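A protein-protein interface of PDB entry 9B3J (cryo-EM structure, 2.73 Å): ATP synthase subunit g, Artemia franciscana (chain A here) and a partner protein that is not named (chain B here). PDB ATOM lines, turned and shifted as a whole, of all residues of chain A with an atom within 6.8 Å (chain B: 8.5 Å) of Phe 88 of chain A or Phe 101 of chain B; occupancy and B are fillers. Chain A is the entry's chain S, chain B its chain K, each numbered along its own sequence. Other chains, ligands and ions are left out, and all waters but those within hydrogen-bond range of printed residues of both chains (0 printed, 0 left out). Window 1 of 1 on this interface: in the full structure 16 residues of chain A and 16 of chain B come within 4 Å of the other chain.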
ATOM      1  N   ILE A  83      31.185  -0.005  -1.501  1.00  0.00           N
ATOM      2  CA  ILE A  83      31.889  -0.269  -0.238  1.00  0.00           C
ATOM      3  C   ILE A  83      31.193  -1.381   0.546  1.00  0.00           C
ATOM      4  O   ILE A  83      31.838  -2.301   1.072  1.00  0.00           O
ATOM      5  CB  ILE A  83      32.003   1.025   0.587  1.00  0.00           C
ATOM      6  CG1 ILE A  83      32.951   2.003  -0.096  1.00  0.00           C
ATOM      7  CG2 ILE A  83      32.457   0.739   1.999  1.00  0.00           C
ATOM      8  CD1 ILE A  83      33.098   3.297   0.642  1.00  0.00           C
ATOM      9  N   ALA A  84      29.865  -1.328   0.609  1.00  0.00           N
ATOM     10  CA  ALA A  84      29.114  -2.375   1.300  1.00  0.00           C
ATOM     11  C   ALA A  84      29.230  -3.723   0.590  1.00  0.00           C
ATOM     12  O   ALA A  84      29.220  -4.778   1.240  1.00  0.00           O
ATOM     13  CB  ALA A  84      27.649  -1.972   1.434  1.00  0.00           C
ATOM     14  N   MET A  85      29.364  -3.715  -0.733  1.00  0.00           N
ATOM     15  CA  MET A  85      29.573  -4.971  -1.442  1.00  0.00           C
ATOM     16  C   MET A  85      30.977  -5.520  -1.213  1.00  0.00           C
ATOM     17  O   MET A  85      31.167  -6.739  -1.205  1.00  0.00           O
ATOM     18  CB  MET A  85      29.287  -4.784  -2.927  1.00  0.00           C
ATOM     19  CG  MET A  85      27.809  -4.778  -3.223  1.00  0.00           C
ATOM     20  SD  MET A  85      27.411  -4.091  -4.829  1.00  0.00           S
ATOM     21  CE  MET A  85      25.623  -4.171  -4.764  1.00  0.00           C
ATOM     22  N   TRP A  86      31.964  -4.641  -1.017  1.00  0.00           N
ATOM     23  CA  TRP A  86      33.283  -5.102  -0.588  1.00  0.00           C
ATOM     24  C   TRP A  86      33.230  -5.703   0.806  1.00  0.00           C
ATOM     25  O   TRP A  86      33.969  -6.647   1.104  1.00  0.00           O
ATOM     26  CB  TRP A  86      34.292  -3.956  -0.623  1.00  0.00           C
ATOM     27  CG  TRP A  86      35.025  -3.849  -1.917  1.00  0.00           C
ATOM     28  CD1 TRP A  86      34.557  -3.321  -3.078  1.00  0.00           C
ATOM     29  CD2 TRP A  86      36.362  -4.279  -2.182  1.00  0.00           C
ATOM     30  NE1 TRP A  86      35.517  -3.398  -4.054  1.00  0.00           N
ATOM     31  CE2 TRP A  86      36.636  -3.982  -3.527  1.00  0.00           C
ATOM     32  CE3 TRP A  86      37.354  -4.883  -1.413  1.00  0.00           C
ATOM     33  CZ2 TRP A  86      37.858  -4.271  -4.119  1.00  0.00           C
ATOM     34  CZ3 TRP A  86      38.566  -5.169  -2.003  1.00  0.00           C
ATOM     35  CH2 TRP A  86      38.808  -4.863  -3.343  1.00  0.00           C
ATOM     36  N   PHE A  87      32.363  -5.165   1.664  1.00  0.00           N
ATOM     37  CA  PHE A  87      32.154  -5.751   2.988  1.00  0.00           C
ATOM     38  C   PHE A  87      31.583  -7.160   2.888  1.00  0.00           C
ATOM     39  O   PHE A  87      31.982  -8.056   3.639  1.00  0.00           O
ATOM     40  CB  PHE A  87      31.232  -4.853   3.809  1.00  0.00           C
ATOM     41  CG  PHE A  87      30.533  -5.553   4.935  1.00  0.00           C
ATOM     42  CD1 PHE A  87      31.193  -5.810   6.117  1.00  0.00           C
ATOM     43  CD2 PHE A  87      29.204  -5.921   4.825  1.00  0.00           C
ATOM     44  CE1 PHE A  87      30.552  -6.444   7.160  1.00  0.00           C
ATOM     45  CE2 PHE A  87      28.560  -6.559   5.863  1.00  0.00           C
ATOM     46  CZ  PHE A  87      29.236  -6.819   7.030  1.00  0.00           C
ATOM     47  N   PHE A  88      30.638  -7.371   1.974  1.00  0.00           N
ATOM     48  CA  PHE A  88      30.074  -8.713   1.820  1.00  0.00           C
ATOM     49  C   PHE A  88      31.031  -9.665   1.115  1.00  0.00           C
ATOM     50  O   PHE A  88      30.978 -10.878   1.347  1.00  0.00           O
ATOM     51  CB  PHE A  88      28.750  -8.652   1.073  1.00  0.00           C
ATOM     52  CG  PHE A  88      27.593  -8.292   1.943  1.00  0.00           C
ATOM     53  CD1 PHE A  88      26.993  -9.248   2.736  1.00  0.00           C
ATOM     54  CD2 PHE A  88      27.109  -6.999   1.974  1.00  0.00           C
ATOM     55  CE1 PHE A  88      25.927  -8.922   3.541  1.00  0.00           C
ATOM     56  CE2 PHE A  88      26.047  -6.666   2.776  1.00  0.00           C
ATOM     57  CZ  PHE A  88      25.454  -7.629   3.561  1.00  0.00           C
ATOM     58  N   VAL A  89      31.901  -9.147   0.248  1.00  0.00           N
ATOM     59  CA  VAL A  89      32.970  -9.970  -0.309  1.00  0.00           C
ATOM     60  C   VAL A  89      33.914 -10.416   0.796  1.00  0.00           C
ATOM     61  O   VAL A  89      34.310 -11.585   0.860  1.00  0.00           O
ATOM     62  CB  VAL A  89      33.707  -9.200  -1.421  1.00  0.00           C
ATOM     63  CG1 VAL A  89      35.055  -9.823  -1.718  1.00  0.00           C
ATOM     64  CG2 VAL A  89      32.862  -9.168  -2.674  1.00  0.00           C
ATOM     65  N   GLY A  90      34.273  -9.495   1.692  1.00  0.00           N
ATOM     66  CA  GLY A  90      35.079  -9.862   2.844  1.00  0.00           C
ATOM     67  C   GLY A  90      34.381 -10.835   3.768  1.00  0.00           C
ATOM     68  O   GLY A  90      35.026 -11.686   4.381  1.00  0.00           O
ATOM     69  N   GLU A  91      33.060 -10.731   3.877  1.00  0.00           N
ATOM     70  CA  GLU A  91      32.312 -11.727   4.632  1.00  0.00           C
ATOM     71  C   GLU A  91      32.346 -13.085   3.945  1.00  0.00           C
ATOM     72  O   GLU A  91      32.379 -14.119   4.620  1.00  0.00           O
ATOM     73  CB  GLU A  91      30.879 -11.251   4.833  1.00  0.00           C
ATOM     74  CG  GLU A  91      30.083 -12.063   5.818  1.00  0.00           C
ATOM     75  CD  GLU A  91      28.862 -11.320   6.308  1.00  0.00           C
ATOM     76  OE1 GLU A  91      28.849 -10.074   6.214  1.00  0.00           O
ATOM     77  OE2 GLU A  91      27.916 -11.979   6.785  1.00  0.00           O
ATOM     78  N   CYS A  92      32.350 -13.101   2.611  1.00  0.00           N
ATOM     79  CA  CYS A  92      32.512 -14.357   1.883  1.00  0.00           C
ATOM     80  C   CYS A  92      33.905 -14.938   2.087  1.00  0.00           C
ATOM     81  O   CYS A  92      34.068 -16.160   2.175  1.00  0.00           O
ATOM     82  CB  CYS A  92      32.239 -14.149   0.395  1.00  0.00           C
ATOM     83  SG  CYS A  92      30.528 -13.781  -0.003  1.00  0.00           S
ATOM     84  N   ILE A  93      34.919 -14.074   2.129  1.00  0.00           N
ATOM     85  CA  ILE A  93      36.286 -14.514   2.393  1.00  0.00           C
ATOM     86  C   ILE A  93      36.388 -15.112   3.791  1.00  0.00           C
ATOM     87  O   ILE A  93      36.969 -16.187   3.986  1.00  0.00           O
ATOM     88  CB  ILE A  93      37.268 -13.342   2.203  1.00  0.00           C
ATOM     89  CG1 ILE A  93      37.404 -12.994   0.720  1.00  0.00           C
ATOM     90  CG2 ILE A  93      38.622 -13.659   2.804  1.00  0.00           C
ATOM     91  CD1 ILE A  93      38.450 -11.941   0.435  1.00  0.00           C
ATOM     92  N   LYS A  95      33.971 -16.381   5.665  1.00  0.00           N
ATOM     93  CA  LYS A  95      33.181 -17.596   5.797  1.00  0.00           C
ATOM     94  C   LYS A  95      33.595 -18.686   4.819  1.00  0.00           C
ATOM     95  O   LYS A  95      33.042 -19.789   4.872  1.00  0.00           O
ATOM     96  CB  LYS A  95      31.695 -17.282   5.616  1.00  0.00           C
ATOM     97  CG  LYS A  95      31.243 -17.096   4.178  1.00  0.00           C
ATOM     98  CD  LYS A  95      29.879 -16.425   4.134  1.00  0.00           C
ATOM     99  CE  LYS A  95      29.390 -16.225   2.715  1.00  0.00           C
ATOM    100  NZ  LYS A  95      28.111 -15.466   2.684  1.00  0.00           N
ATOM    101  N   LEU B  94      32.148  -3.047  -8.761  1.00  0.00           N
ATOM    102  CA  LEU B  94      30.791  -2.896  -8.245  1.00  0.00           C
ATOM    103  C   LEU B  94      29.881  -4.003  -8.759  1.00  0.00           C
ATOM    104  O   LEU B  94      29.086  -4.567  -8.000  1.00  0.00           O
ATOM    105  CB  LEU B  94      30.237  -1.527  -8.632  1.00  0.00           C
ATOM    106  CG  LEU B  94      28.753  -1.269  -8.377  1.00  0.00           C
ATOM    107  CD1 LEU B  94      28.459  -1.246  -6.902  1.00  0.00           C
ATOM    108  CD2 LEU B  94      28.330   0.033  -9.011  1.00  0.00           C
ATOM    109  N   GLY B  95      29.993  -4.331 -10.046  1.00  0.00           N
ATOM    110  CA  GLY B  95      29.249  -5.458 -10.581  1.00  0.00           C
ATOM    111  C   GLY B  95      29.708  -6.790 -10.026  1.00  0.00           C
ATOM    112  O   GLY B  95      28.894  -7.697  -9.820  1.00  0.00           O
ATOM    113  N   ALA B  96      31.012  -6.926  -9.770  1.00  0.00           N
ATOM    114  CA  ALA B  96      31.526  -8.151  -9.168  1.00  0.00           C
ATOM    115  C   ALA B  96      31.040  -8.313  -7.735  1.00  0.00           C
ATOM    116  O   ALA B  96      30.641  -9.413  -7.330  1.00  0.00           O
ATOM    117  CB  ALA B  96      33.050  -8.158  -9.222  1.00  0.00           C
ATOM    118  N   GLY B  97      31.059  -7.234  -6.952  1.00  0.00           N
ATOM    119  CA  GLY B  97      30.524  -7.293  -5.608  1.00  0.00           C
ATOM    120  C   GLY B  97      29.029  -7.519  -5.578  1.00  0.00           C
ATOM    121  O   GLY B  97      28.522  -8.187  -4.675  1.00  0.00           O
ATOM    122  N   ALA B  98      28.306  -6.980  -6.564  1.00  0.00           N
ATOM    123  CA  ALA B  98      26.867  -7.207  -6.637  1.00  0.00           C
ATOM    124  C   ALA B  98      26.548  -8.664  -6.933  1.00  0.00           C
ATOM    125  O   ALA B  98      25.664  -9.252  -6.301  1.00  0.00           O
ATOM    126  CB  ALA B  98      26.247  -6.305  -7.698  1.00  0.00           C
ATOM    127  N   LEU B  99      27.251  -9.261  -7.898  1.00  0.00           N
ATOM    128  CA  LEU B  99      27.001 -10.661  -8.222  1.00  0.00           C
ATOM    129  C   LEU B  99      27.421 -11.576  -7.083  1.00  0.00           C
ATOM    130  O   LEU B  99      26.750 -12.579  -6.798  1.00  0.00           O
ATOM    131  CB  LEU B  99      27.729 -11.040  -9.505  1.00  0.00           C
ATOM    132  CG  LEU B  99      27.414 -12.436 -10.035  1.00  0.00           C
ATOM    133  CD1 LEU B  99      25.943 -12.537 -10.383  1.00  0.00           C
ATOM    134  CD2 LEU B  99      28.281 -12.759 -11.236  1.00  0.00           C
ATOM    135  N   THR B 100      28.521 -11.240  -6.407  1.00  0.00           N
ATOM    136  CA  THR B 100      28.937 -12.033  -5.260  1.00  0.00           C
ATOM    137  C   THR B 100      27.948 -11.898  -4.111  1.00  0.00           C
ATOM    138  O   THR B 100      27.683 -12.874  -3.410  1.00  0.00           O
ATOM    139  CB  THR B 100      30.337 -11.627  -4.814  1.00  0.00           C
ATOM    140  OG1 THR B 100      31.191 -11.529  -5.960  1.00  0.00           O
ATOM    141  CG2 THR B 100      30.909 -12.666  -3.874  1.00  0.00           C
ATOM    142  N   PHE B 101      27.378 -10.706  -3.912  1.00  0.00           N
ATOM    143  CA  PHE B 101      26.403 -10.532  -2.839  1.00  0.00           C
ATOM    144  C   PHE B 101      25.091 -11.241  -3.149  1.00  0.00           C
ATOM    145  O   PHE B 101      24.443 -11.771  -2.240  1.00  0.00           O
ATOM    146  CB  PHE B 101      26.148  -9.051  -2.584  1.00  0.00           C
ATOM    147  CG  PHE B 101      24.911  -8.792  -1.788  1.00  0.00           C
ATOM    148  CD1 PHE B 101      24.839  -9.164  -0.462  1.00  0.00           C
ATOM    149  CD2 PHE B 101      23.813  -8.188  -2.367  1.00  0.00           C
ATOM    150  CE1 PHE B 101      23.700  -8.934   0.268  1.00  0.00           C
ATOM    151  CE2 PHE B 101      22.671  -7.953  -1.637  1.00  0.00           C
ATOM    152  CZ  PHE B 101      22.616  -8.326  -0.318  1.00  0.00           C
ATOM    153  N   LEU B 102      24.664 -11.235  -4.412  1.00  0.00           N
ATOM    154  CA  LEU B 102      23.463 -11.980  -4.773  1.00  0.00           C
ATOM    155  C   LEU B 102      23.668 -13.475  -4.586  1.00  0.00           C
ATOM    156  O   LEU B 102      22.782 -14.167  -4.076  1.00  0.00           O
ATOM    157  CB  LEU B 102      23.055 -11.684  -6.211  1.00  0.00           C
ATOM    158  CG  LEU B 102      22.549 -10.283  -6.518  1.00  0.00           C
ATOM    159  CD1 LEU B 102      22.008 -10.250  -7.926  1.00  0.00           C
ATOM    160  CD2 LEU B 102      21.491  -9.879  -5.520  1.00  0.00           C
ATOM    161  N   LEU B 103      24.826 -13.991  -4.982  1.00  0.00           N
ATOM    162  CA  LEU B 103      25.083 -15.404  -4.756  1.00  0.00           C
ATOM    163  C   LEU B 103      25.460 -15.716  -3.312  1.00  0.00           C
ATOM    164  O   LEU B 103      25.455 -16.889  -2.932  1.00  0.00           O
ATOM    165  CB  LEU B 103      26.182 -15.893  -5.699  1.00  0.00           C
ATOM    166  CG  LEU B 103      25.897 -15.803  -7.198  1.00  0.00           C
ATOM    167  CD1 LEU B 103      27.123 -16.195  -7.994  1.00  0.00           C
ATOM    168  CD2 LEU B 103      24.737 -16.688  -7.570  1.00  0.00           C
ATOM    169  N   SER B 104      25.778 -14.708  -2.500  1.00  0.00           N
ATOM    170  CA  SER B 104      26.145 -14.954  -1.110  1.00  0.00           C
ATOM    171  C   SER B 104      24.907 -15.144  -0.253  1.00  0.00           C
ATOM    172  O   SER B 104      24.698 -16.212   0.332  1.00  0.00           O
ATOM    173  CB  SER B 104      26.987 -13.800  -0.561  1.00  0.00           C
ATOM    174  OG  SER B 104      27.428 -14.073   0.760  1.00  0.00           O
ATOM    175  N   LYS B 105      24.063 -14.122  -0.183  1.00  0.00           N
ATOM    176  CA  LYS B 105      22.826 -14.196   0.572  1.00  0.00           C
ATOM    177  C   LYS B 105      21.740 -14.979  -0.150  1.00  0.00           C
ATOM    178  O   LYS B 105      20.610 -15.013   0.347  1.00  0.00           O
ATOM    179  CB  LYS B 105      22.321 -12.792   0.895  1.00  0.00           C
ATOM    180  CG  LYS B 105      22.996 -12.144   2.091  1.00  0.00           C
ATOM    181  CD  LYS B 105      22.091 -11.074   2.701  1.00  0.00           C
ATOM    182  CE  LYS B 105      22.632 -10.536   4.018  1.00  0.00           C
ATOM    183  NZ  LYS B 105      21.716  -9.529   4.615  1.00  0.00           N
ATOM    184  N   GLU B 106      22.056 -15.581  -1.301  1.00  0.00           N
ATOM    185  CA  GLU B 106      21.135 -16.406  -2.085  1.00  0.00           C
ATOM    186  C   GLU B 106      19.879 -15.649  -2.488  1.00  0.00           C
ATOM    187  O   GLU B 106      18.799 -16.230  -2.586  1.00  0.00           O
ATOM    188  CB  GLU B 106      20.767 -17.693  -1.351  1.00  0.00           C
ATOM    189  CG  GLU B 106      21.693 -18.837  -1.657  1.00  0.00           C
ATOM    190  CD  GLU B 106      21.372 -20.061  -0.840  1.00  0.00           C
ATOM    191  OE1 GLU B 106      20.812 -19.907   0.264  1.00  0.00           O
ATOM    192  OE2 GLU B 106      21.677 -21.179  -1.304  1.00  0.00           O
ATOM    193  N   ILE B 107      20.008 -14.339  -2.700  1.00  0.00           N
ATOM    194  CA  ILE B 107      18.938 -13.590  -3.342  1.00  0.00           C
ATOM    195  C   ILE B 107      18.749 -14.082  -4.767  1.00  0.00           C
ATOM    196  O   ILE B 107      17.622 -14.307  -5.220  1.00  0.00           O
ATOM    197  CB  ILE B 107      19.243 -12.086  -3.294  1.00  0.00           C
ATOM    198  CG1 ILE B 107      19.384 -11.633  -1.847  1.00  0.00           C
ATOM    199  CG2 ILE B 107      18.157 -11.310  -3.981  1.00  0.00           C
ATOM    200  CD1 ILE B 107      19.729 -10.181  -1.714  1.00  0.00           C
ATOM    201  N   TYR B 108      19.847 -14.271  -5.486  1.00  0.00           N
ATOM    202  CA  TYR B 108      19.826 -14.946  -6.777  1.00  0.00           C
ATOM    203  C   TYR B 108      20.091 -16.418  -6.523  1.00  0.00           C
ATOM    204  O   TYR B 108      21.223 -16.807  -6.230  1.00  0.00           O
ATOM    205  CB  TYR B 108      20.864 -14.352  -7.723  1.00  0.00           C
ATOM    206  CG  TYR B 108      20.861 -14.982  -9.095  1.00  0.00           C
ATOM    207  CD1 TYR B 108      20.019 -14.517 -10.088  1.00  0.00           C
ATOM    208  CD2 TYR B 108      21.701 -16.040  -9.397  1.00  0.00           C
ATOM    209  CE1 TYR B 108      20.009 -15.088 -11.332  1.00  0.00           C
ATOM    210  CE2 TYR B 108      21.697 -16.617 -10.638  1.00  0.00           C
ATOM    211  CZ  TYR B 108      20.851 -16.138 -11.600  1.00  0.00           C
ATOM    212  OH  TYR B 108      20.854 -16.721 -12.840  1.00  0.00           O
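Among the printed residues, merely in contact across the chains: Phe 88 of chain A with Lys 105 of chain B, Phe 88 of chain A with Phe 101 of chain B and Met 85 of chain A with Gly 97 of chain B.
OG of Ser 104 of chain B lies within hydrogen-bond range of SG of Cys 92 of chain A (3.2 Å). The side-chain hydroxyl (OG) of Ser 104 of chain B lies within hydrogen-bond range of the side-chain amino group (NZ) of Lys 95 of chain A. The backbone NH of Ala 98 of chain B is in hydrogen-bond range of the side-chain sulfur of Met 85 of chain A (3.5 Å). SD of Met 85 of chain A lies close to O of Leu 94 of chain B (3.6 Å).
Of the 12 printed residues of chain A, 4 touch a printed residue of chain B. Among the printed residues, 7 pairs touch across the chains.
Of the printed residues of chain B, Phe 88 of chain A touches Phe 101 and Lys 105. Val 89 of chain A touches none of the printed residues of chain B. Of the printed residues of chain B, Cys 92 of chain A touches Ser 104. Printed residues of chain A within 4 Å of Leu 94 of chain B: Met 85 (3.6 Å). Of the printed residues of chain A, Gly 97 of chain B touches Met 85. Of the printed residues of chain A, Ala 98 of chain B touches Met 85. Of the printed residues of chain A, Phe 101 of chain B touches Phe 88 (3.8 Å). Of the printed residues of chain A, Lys 105 of chain B touches Phe 88. The nearest residue of chain A that does not touch Phe 101 of chain B is Met 85 of chain A (4.6 Å). The nearest printed residue of chain B that does not touch Met 85 of chain A is Phe 101 of chain B (4.6 Å).
The backbone carbonyl oxygen (O) of Phe 88 of chain A is in hydrogen-bond range of the side-chain sulfur (SG) of Cys 92 of chain A, at 3.2 Å.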
